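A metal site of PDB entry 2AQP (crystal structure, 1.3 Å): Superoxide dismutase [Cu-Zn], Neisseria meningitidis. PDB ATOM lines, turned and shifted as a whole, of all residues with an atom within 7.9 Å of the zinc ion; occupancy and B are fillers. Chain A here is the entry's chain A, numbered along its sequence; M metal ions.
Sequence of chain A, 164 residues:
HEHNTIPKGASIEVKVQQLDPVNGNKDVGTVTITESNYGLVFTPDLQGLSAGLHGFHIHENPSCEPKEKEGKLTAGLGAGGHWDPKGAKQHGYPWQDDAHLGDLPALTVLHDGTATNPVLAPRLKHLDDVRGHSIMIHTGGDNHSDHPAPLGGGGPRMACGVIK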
ATOM      1  N   PHE A  56       3.708  -8.877  26.660  1.00  0.00           N
ATOM      2  CA  PHE A  56       2.810  -9.768  25.971  1.00  0.00           C
ATOM      3  C   PHE A  56       3.514 -10.371  24.773  1.00  0.00           C
ATOM      4  O   PHE A  56       3.832  -9.624  23.848  1.00  0.00           O
ATOM      5  CB  PHE A  56       1.589  -8.962  25.556  1.00  0.00           C
ATOM      6  CG  PHE A  56       0.343  -9.656  25.089  1.00  0.00           C
ATOM      7  CD1 PHE A  56      -0.171 -10.773  25.732  1.00  0.00           C
ATOM      8  CD2 PHE A  56      -0.375  -9.162  24.006  1.00  0.00           C
ATOM      9  CE1 PHE A  56      -1.342 -11.344  25.312  1.00  0.00           C
ATOM     10  CE2 PHE A  56      -1.556  -9.744  23.604  1.00  0.00           C
ATOM     11  CZ  PHE A  56      -2.058 -10.818  24.269  1.00  0.00           C
ATOM     12  N   HIS A  57       3.797 -11.672  24.859  1.00  0.00           N
ATOM     13  CA  HIS A  57       4.590 -12.301  23.782  1.00  0.00           C
ATOM     14  C   HIS A  57       4.103 -13.729  23.522  1.00  0.00           C
ATOM     15  O   HIS A  57       3.558 -14.391  24.380  1.00  0.00           O
ATOM     16  CB  HIS A  57       6.078 -12.403  24.109  1.00  0.00           C
ATOM     17  CG  HIS A  57       6.615 -11.347  25.014  1.00  0.00           C
ATOM     18  ND1 HIS A  57       6.937 -11.569  26.331  1.00  0.00           N
ATOM     19  CD2 HIS A  57       6.803 -10.025  24.772  1.00  0.00           C
ATOM     20  CE1 HIS A  57       7.349 -10.409  26.842  1.00  0.00           C
ATOM     21  NE2 HIS A  57       7.277  -9.433  25.936  1.00  0.00           N
ATOM     22  N   ILE A  58       4.396 -14.167  22.275  1.00  0.00           N
ATOM     23  CA  ILE A  58       4.317 -15.587  21.980  1.00  0.00           C
ATOM     24  C   ILE A  58       5.595 -16.273  22.420  1.00  0.00           C
ATOM     25  O   ILE A  58       6.676 -15.808  22.070  1.00  0.00           O
ATOM     26  CB  ILE A  58       4.100 -15.784  20.477  1.00  0.00           C
ATOM     27  CG1 ILE A  58       2.847 -15.069  19.952  1.00  0.00           C
ATOM     28  CG2 ILE A  58       4.071 -17.260  20.157  1.00  0.00           C
ATOM     29  CD1 ILE A  58       1.564 -15.692  20.453  1.00  0.00           C
ATOM     30  N   HIS A  59       5.389 -17.345  23.198  1.00  0.00           N
ATOM     31  CA  HIS A  59       6.561 -18.145  23.595  1.00  0.00           C
ATOM     32  C   HIS A  59       6.606 -19.437  22.819  1.00  0.00           C
ATOM     33  O   HIS A  59       5.661 -19.855  22.195  1.00  0.00           O
ATOM     34  CB  HIS A  59       6.563 -18.410  25.098  1.00  0.00           C
ATOM     35  CG  HIS A  59       6.957 -17.217  25.887  1.00  0.00           C
ATOM     36  ND1 HIS A  59       7.968 -17.231  26.802  1.00  0.00           N
ATOM     37  CD2 HIS A  59       6.513 -15.911  25.897  1.00  0.00           C
ATOM     38  CE1 HIS A  59       8.105 -16.025  27.358  1.00  0.00           C
ATOM     39  NE2 HIS A  59       7.242 -15.193  26.838  1.00  0.00           N
ATOM     40  N   GLY A  81      11.227 -19.865  25.857  1.00  0.00           N
ATOM     41  CA  GLY A  81      11.544 -18.487  25.600  1.00  0.00           C
ATOM     42  C   GLY A  81      10.658 -17.832  24.559  1.00  0.00           C
ATOM     43  O   GLY A  81       9.681 -18.429  24.092  1.00  0.00           O
ATOM     44  N   HIS A  82      11.018 -16.565  24.262  1.00  0.00           N
ATOM     45  CA  HIS A  82      10.279 -15.848  23.238  1.00  0.00           C
ATOM     46  C   HIS A  82      10.342 -16.619  21.929  1.00  0.00           C
ATOM     47  O   HIS A  82      11.381 -17.110  21.518  1.00  0.00           O
ATOM     48  CB  HIS A  82      10.860 -14.441  23.134  1.00  0.00           C
ATOM     49  CG  HIS A  82      10.520 -13.533  24.276  1.00  0.00           C
ATOM     50  ND1 HIS A  82      10.528 -12.164  24.185  1.00  0.00           N
ATOM     51  CD2 HIS A  82      10.203 -13.812  25.569  1.00  0.00           C
ATOM     52  CE1 HIS A  82      10.202 -11.628  25.341  1.00  0.00           C
ATOM     53  NE2 HIS A  82      10.001 -12.626  26.216  1.00  0.00           N
ATOM     54  N   TRP A  83       9.198 -16.764  21.237  1.00  0.00           N
ATOM     55  CA  TRP A  83       9.215 -17.466  19.957  1.00  0.00           C
ATOM     56  C   TRP A  83      10.077 -16.711  18.955  1.00  0.00           C
ATOM     57  O   TRP A  83       9.862 -15.516  18.701  1.00  0.00           O
ATOM     58  CB  TRP A  83       7.767 -17.609  19.505  1.00  0.00           C
ATOM     59  CG  TRP A  83       7.528 -18.430  18.271  1.00  0.00           C
ATOM     60  CD1 TRP A  83       8.015 -19.642  17.890  1.00  0.00           C
ATOM     61  CD2 TRP A  83       6.657 -18.025  17.188  1.00  0.00           C
ATOM     62  NE1 TRP A  83       7.520 -20.029  16.679  1.00  0.00           N
ATOM     63  CE2 TRP A  83       6.672 -19.043  16.222  1.00  0.00           C
ATOM     64  CE3 TRP A  83       5.876 -16.901  16.989  1.00  0.00           C
ATOM     65  CZ2 TRP A  83       5.926 -18.960  15.037  1.00  0.00           C
ATOM     66  CZ3 TRP A  83       5.133 -16.790  15.835  1.00  0.00           C
ATOM     67  CH2 TRP A  83       5.175 -17.820  14.877  1.00  0.00           C
ATOM     68  N   ASP A  84      11.068 -17.394  18.374  1.00  0.00           N
ATOM     69  CA  ASP A  84      12.108 -16.734  17.558  1.00  0.00           C
ATOM     70  C   ASP A  84      12.487 -17.655  16.412  1.00  0.00           C
ATOM     71  O   ASP A  84      13.651 -18.068  16.283  1.00  0.00           O
ATOM     72  CB  ASP A  84      13.300 -16.319  18.421  1.00  0.00           C
ATOM     73  CG  ASP A  84      14.337 -15.439  17.676  1.00  0.00           C
ATOM     74  OD1 ASP A  84      13.963 -15.095  16.576  1.00  0.00           O
ATOM     75  OD2 ASP A  84      15.402 -15.330  18.191  1.00  0.00           O
ATOM     76  N   LYS A  89      17.390 -13.444  17.764  1.00  0.00           N
ATOM     77  CA  LYS A  89      18.157 -13.552  18.998  1.00  0.00           C
ATOM     78  C   LYS A  89      18.253 -12.223  19.735  1.00  0.00           C
ATOM     79  O   LYS A  89      19.218 -11.921  20.425  1.00  0.00           O
ATOM     80  CB  LYS A  89      19.561 -14.146  18.772  1.00  0.00           C
ATOM     81  CG  LYS A  89      19.582 -15.574  18.312  1.00  0.00           C
ATOM     82  CD  LYS A  89      20.982 -16.072  17.928  1.00  0.00           C
ATOM     83  CE  LYS A  89      21.010 -17.528  17.518  1.00  0.00           C
ATOM     84  NZ  LYS A  89      21.957 -17.720  16.374  1.00  0.00           N
ATOM     85  N   GLN A  90      17.200 -11.425  19.630  1.00  0.00           N
ATOM     86  CA  GLN A  90      17.077 -10.222  20.465  1.00  0.00           C
ATOM     87  C   GLN A  90      15.630  -9.782  20.524  1.00  0.00           C
ATOM     88  O   GLN A  90      14.842 -10.021  19.621  1.00  0.00           O
ATOM     89  CB  GLN A  90      17.933  -9.095  19.908  1.00  0.00           C
ATOM     90  CG  GLN A  90      17.461  -8.602  18.548  1.00  0.00           C
ATOM     91  CD  GLN A  90      18.352  -7.556  17.901  1.00  0.00           C
ATOM     92  OE1 GLN A  90      18.182  -7.129  16.726  1.00  0.00           O
ATOM     93  NE2 GLN A  90      19.338  -7.079  18.631  1.00  0.00           N
ATOM     94  N   HIS A  91      15.288  -9.135  21.629  1.00  0.00           N
ATOM     95  CA  HIS A  91      13.955  -8.699  21.877  1.00  0.00           C
ATOM     96  C   HIS A  91      13.768  -7.297  21.325  1.00  0.00           C
ATOM     97  O   HIS A  91      14.687  -6.464  21.406  1.00  0.00           O
ATOM     98  CB  HIS A  91      13.727  -8.742  23.420  1.00  0.00           C
ATOM     99  CG  HIS A  91      12.323  -8.374  23.773  1.00  0.00           C
ATOM    100  ND1 HIS A  91      11.241  -9.142  23.490  1.00  0.00           N
ATOM    101  CD2 HIS A  91      11.847  -7.223  24.338  1.00  0.00           C
ATOM    102  CE1 HIS A  91      10.136  -8.510  23.877  1.00  0.00           C
ATOM    103  NE2 HIS A  91      10.462  -7.351  24.408  1.00  0.00           N
ATOM    104  N   GLY A  92      12.602  -7.015  20.737  1.00  0.00           N
ATOM    105  CA  GLY A  92      12.381  -5.695  20.138  1.00  0.00           C
ATOM    106  C   GLY A  92      10.909  -5.378  20.013  1.00  0.00           C
ATOM    107  O   GLY A  92      10.046  -5.827  20.774  1.00  0.00           O
ATOM    108  N   TYR A  93      10.603  -4.606  19.019  1.00  0.00           N
ATOM    109  CA  TYR A  93       9.364  -3.955  18.748  1.00  0.00           C
ATOM    110  C   TYR A  93       8.493  -4.881  17.907  1.00  0.00           C
ATOM    111  O   TYR A  93       9.030  -5.685  17.149  1.00  0.00           O
ATOM    112  CB  TYR A  93       9.500  -2.604  18.052  1.00  0.00           C
ATOM    113  CG  TYR A  93      10.098  -1.510  18.881  1.00  0.00           C
ATOM    114  CD1 TYR A  93       9.333  -0.779  19.776  1.00  0.00           C
ATOM    115  CD2 TYR A  93      11.448  -1.180  18.766  1.00  0.00           C
ATOM    116  CE1 TYR A  93       9.889   0.218  20.521  1.00  0.00           C
ATOM    117  CE2 TYR A  93      12.022  -0.192  19.516  1.00  0.00           C
ATOM    118  CZ  TYR A  93      11.236   0.530  20.392  1.00  0.00           C
ATOM    119  OH  TYR A  93      11.814   1.506  21.149  1.00  0.00           O
ATOM    120  N   ALA A  99      13.721  -8.542  15.415  1.00  0.00           N
ATOM    121  CA  ALA A  99      13.268  -8.934  16.732  1.00  0.00           C
ATOM    122  C   ALA A  99      12.566 -10.276  16.727  1.00  0.00           C
ATOM    123  O   ALA A  99      12.083 -10.686  15.678  1.00  0.00           O
ATOM    124  CB  ALA A  99      12.322  -7.885  17.326  1.00  0.00           C
ATOM    125  N   HIS A 100      12.530 -10.945  17.892  1.00  0.00           N
ATOM    126  CA  HIS A 100      11.742 -12.160  18.030  1.00  0.00           C
ATOM    127  C   HIS A 100      10.378 -12.019  17.365  1.00  0.00           C
ATOM    128  O   HIS A 100       9.690 -11.030  17.589  1.00  0.00           O
ATOM    129  CB  HIS A 100      11.464 -12.508  19.478  1.00  0.00           C
ATOM    130  CG  HIS A 100      12.591 -12.548  20.423  1.00  0.00           C
ATOM    131  ND1 HIS A 100      12.561 -11.918  21.674  1.00  0.00           N
ATOM    132  CD2 HIS A 100      13.768 -13.192  20.285  1.00  0.00           C
ATOM    133  CE1 HIS A 100      13.722 -12.184  22.265  1.00  0.00           C
ATOM    134  NE2 HIS A 100      14.453 -12.950  21.435  1.00  0.00           N
ATOM    135  N   LEU A 101      10.022 -12.975  16.535  1.00  0.00           N
ATOM    136  CA  LEU A 101       8.724 -12.922  15.899  1.00  0.00           C
ATOM    137  C   LEU A 101       7.558 -12.915  16.887  1.00  0.00           C
ATOM    138  O   LEU A 101       6.477 -12.419  16.572  1.00  0.00           O
ATOM    139  CB  LEU A 101       8.610 -14.069  14.909  1.00  0.00           C
ATOM    140  CG  LEU A 101       7.496 -13.974  13.888  1.00  0.00           C
ATOM    141  CD1 LEU A 101       7.553 -12.737  13.013  1.00  0.00           C
ATOM    142  CD2 LEU A 101       7.542 -15.196  12.935  1.00  0.00           C
ATOM    143  N   GLY A 102       7.789 -13.442  18.086  1.00  0.00           N
ATOM    144  CA  GLY A 102       6.757 -13.450  19.098  1.00  0.00           C
ATOM    145  C   GLY A 102       6.587 -12.171  19.855  1.00  0.00           C
ATOM    146  O   GLY A 102       5.741 -12.147  20.775  1.00  0.00           O
ATOM    147  N   ASP A 103       7.328 -11.114  19.517  1.00  0.00           N
ATOM    148  CA  ASP A 103       7.177  -9.848  20.270  1.00  0.00           C
ATOM    149  C   ASP A 103       5.929  -9.103  19.854  1.00  0.00           C
ATOM    150  O   ASP A 103       5.838  -8.511  18.739  1.00  0.00           O
ATOM    151  CB  ASP A 103       8.450  -9.025  20.081  1.00  0.00           C
ATOM    152  CG  ASP A 103       9.667  -9.662  20.733  1.00  0.00           C
ATOM    153  OD1 ASP A 103       9.491 -10.621  21.540  1.00  0.00           O
ATOM    154  OD2 ASP A 103      10.788  -9.200  20.398  1.00  0.00           O
ATOM    155  N   LEU A 104       4.920  -9.050  20.719  1.00  0.00           N
ATOM    156  CA  LEU A 104       3.670  -8.400  20.483  1.00  0.00           C
ATOM    157  C   LEU A 104       3.602  -7.062  21.176  1.00  0.00           C
ATOM    158  O   LEU A 104       4.399  -6.782  22.067  1.00  0.00           O
ATOM    159  CB  LEU A 104       2.506  -9.236  21.027  1.00  0.00           C
ATOM    160  CG  LEU A 104       2.465 -10.736  20.674  1.00  0.00           C
ATOM    161  CD1 LEU A 104       1.355 -11.399  21.455  1.00  0.00           C
ATOM    162  CD2 LEU A 104       2.320 -10.940  19.143  1.00  0.00           C
ATOM    163  N   ARG A 123       3.834  -8.286  11.982  1.00  0.00           N
ATOM    164  CA  ARG A 123       4.693  -9.310  11.336  1.00  0.00           C
ATOM    165  C   ARG A 123       4.108 -10.713  11.300  1.00  0.00           C
ATOM    166  O   ARG A 123       4.697 -11.601  10.706  1.00  0.00           O
ATOM    167  CB  ARG A 123       6.041  -9.367  12.068  1.00  0.00           C
ATOM    168  CG  ARG A 123       6.754  -8.055  11.907  1.00  0.00           C
ATOM    169  CD  ARG A 123       8.110  -8.056  12.539  1.00  0.00           C
ATOM    170  NE  ARG A 123       8.222  -8.061  13.980  1.00  0.00           N
ATOM    171  CZ  ARG A 123       8.933  -8.860  14.774  1.00  0.00           C
ATOM    172  NH1 ARG A 123       9.673  -9.879  14.316  1.00  0.00           N
ATOM    173  NH2 ARG A 123       8.851  -8.608  16.099  1.00  0.00           N
ATOM    174  N   ASP A 142       7.056  -3.821  28.963  1.00  0.00           N
ATOM    175  CA  ASP A 142       7.862  -4.175  27.791  1.00  0.00           C
ATOM    176  C   ASP A 142       8.350  -2.901  27.127  1.00  0.00           C
ATOM    177  O   ASP A 142       7.637  -2.223  26.389  1.00  0.00           O
ATOM    178  CB  ASP A 142       7.071  -5.042  26.839  1.00  0.00           C
ATOM    179  CG  ASP A 142       7.931  -5.739  25.780  1.00  0.00           C
ATOM    180  OD1 ASP A 142       9.122  -5.354  25.639  1.00  0.00           O
ATOM    181  OD2 ASP A 142       7.385  -6.668  25.146  1.00  0.00           O
ATOM    182  N   HIS A 144      10.547  -3.071  24.786  1.00  0.00           N
ATOM    183  CA  HIS A 144      10.942  -3.508  23.461  1.00  0.00           C
ATOM    184  C   HIS A 144      12.439  -3.441  23.257  1.00  0.00           C
ATOM    185  O   HIS A 144      12.902  -3.144  22.155  1.00  0.00           O
ATOM    186  CB  HIS A 144      10.161  -2.727  22.366  1.00  0.00           C
ATOM    187  CG  HIS A 144       8.697  -2.989  22.508  1.00  0.00           C
ATOM    188  ND1 HIS A 144       8.081  -4.206  22.355  1.00  0.00           N
ATOM    189  CD2 HIS A 144       7.671  -2.150  22.816  1.00  0.00           C
ATOM    190  CE1 HIS A 144       6.776  -4.113  22.567  1.00  0.00           C
ATOM    191  NE2 HIS A 144       6.480  -2.841  22.841  1.00  0.00           N
ATOM    192  N   SER A 145      13.209  -3.771  24.295  1.00  0.00           N
ATOM    193  CA  SER A 145      14.653  -3.829  24.205  1.00  0.00           C
ATOM    194  C   SER A 145      15.132  -4.847  25.241  1.00  0.00           C
ATOM    195  O   SER A 145      14.396  -5.164  26.196  1.00  0.00           O
ATOM    196  CB  SER A 145      15.229  -2.469  24.483  1.00  0.00           C
ATOM    197  OG  SER A 145      16.655  -2.496  24.548  1.00  0.00           O
ATOM    198  N   ASP A 146      16.341  -5.334  25.073  1.00  0.00           N
ATOM    199  CA  ASP A 146      17.012  -6.090  26.117  1.00  0.00           C
ATOM    200  C   ASP A 146      17.826  -5.208  27.050  1.00  0.00           C
ATOM    201  O   ASP A 146      18.525  -5.720  27.935  1.00  0.00           O
ATOM    202  CB  ASP A 146      17.946  -7.147  25.515  1.00  0.00           C
ATOM    203  CG  ASP A 146      17.158  -8.288  24.889  1.00  0.00           C
ATOM    204  OD1 ASP A 146      16.328  -8.897  25.604  1.00  0.00           O
ATOM    205  OD2 ASP A 146      17.378  -8.577  23.694  1.00  0.00           O
ATOM    206  N   LEU A 151      14.626  -8.795  27.840  1.00  0.00           N
ATOM    207  CA  LEU A 151      13.280  -9.149  27.418  1.00  0.00           C
ATOM    208  C   LEU A 151      12.256  -8.102  27.805  1.00  0.00           C
ATOM    209  O   LEU A 151      11.111  -8.389  28.179  1.00  0.00           O
ATOM    210  CB  LEU A 151      12.939 -10.525  27.961  1.00  0.00           C
ATOM    211  CG  LEU A 151      13.898 -11.641  27.541  1.00  0.00           C
ATOM    212  CD1 LEU A 151      13.574 -12.953  28.243  1.00  0.00           C
ATOM    213  CD2 LEU A 151      13.891 -11.842  26.048  1.00  0.00           C
ATOM    214  N   GLY A 152      12.686  -6.844  27.642  1.00  0.00           N
ATOM    215  CA  GLY A 152      11.817  -5.711  27.813  1.00  0.00           C
ATOM    216  C   GLY A 152      11.490  -5.363  29.236  1.00  0.00           C
ATOM    217  O   GLY A 152      10.655  -4.485  29.448  1.00  0.00           O
HETATM  218 ZN    ZN M   1      11.025 -10.988  22.613  1.00  0.00          ZN
HETATM  219 CU    CU M   2       7.050 -13.299  27.191  1.00  0.00          CU
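NE2 of His 91 lies within hydrogen-bond range of OD1 of Asp 142 (2.7 Å).
A ring nitrogen (NE2) of His 82 lies close to a ring nitrogen (ND1) of His 57.
The backbone NH (N) of His 91 sits at hydrogen-bond distance from the side-chain carboxylate (OD2) of Asp 146, 3.0 Å away.
N of Gly 92 is in hydrogen-bond range of OD2 of Asp 103 (2.9 Å).
The guanidinium group (NH2) of Arg 123 is in hydrogen-bond range of the backbone carbonyl oxygen (O) of His 100 (3.0 Å).
N of His 100 is in hydrogen-bond range of O of Gln 90, at 3.0 Å.
Four residues have an atom within 4 Å of the zinc ion: His 82, His 91, His 100 and Asp 103.
The nearest printed residue that does not touch the zinc ion is Leu 151 (4.6 Å).
The zinc ion is bound by the side-chain carboxylate (OD1) of Asp 103 (1.9 Å), a ring nitrogen (ND1) of His 82 (2.0 Å), a ring nitrogen (ND1) of His 100 (2.0 Å) and a ring nitrogen (ND1) of His 91 (2.1 Å).
The zinc ion has four donor atoms within binding distance.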
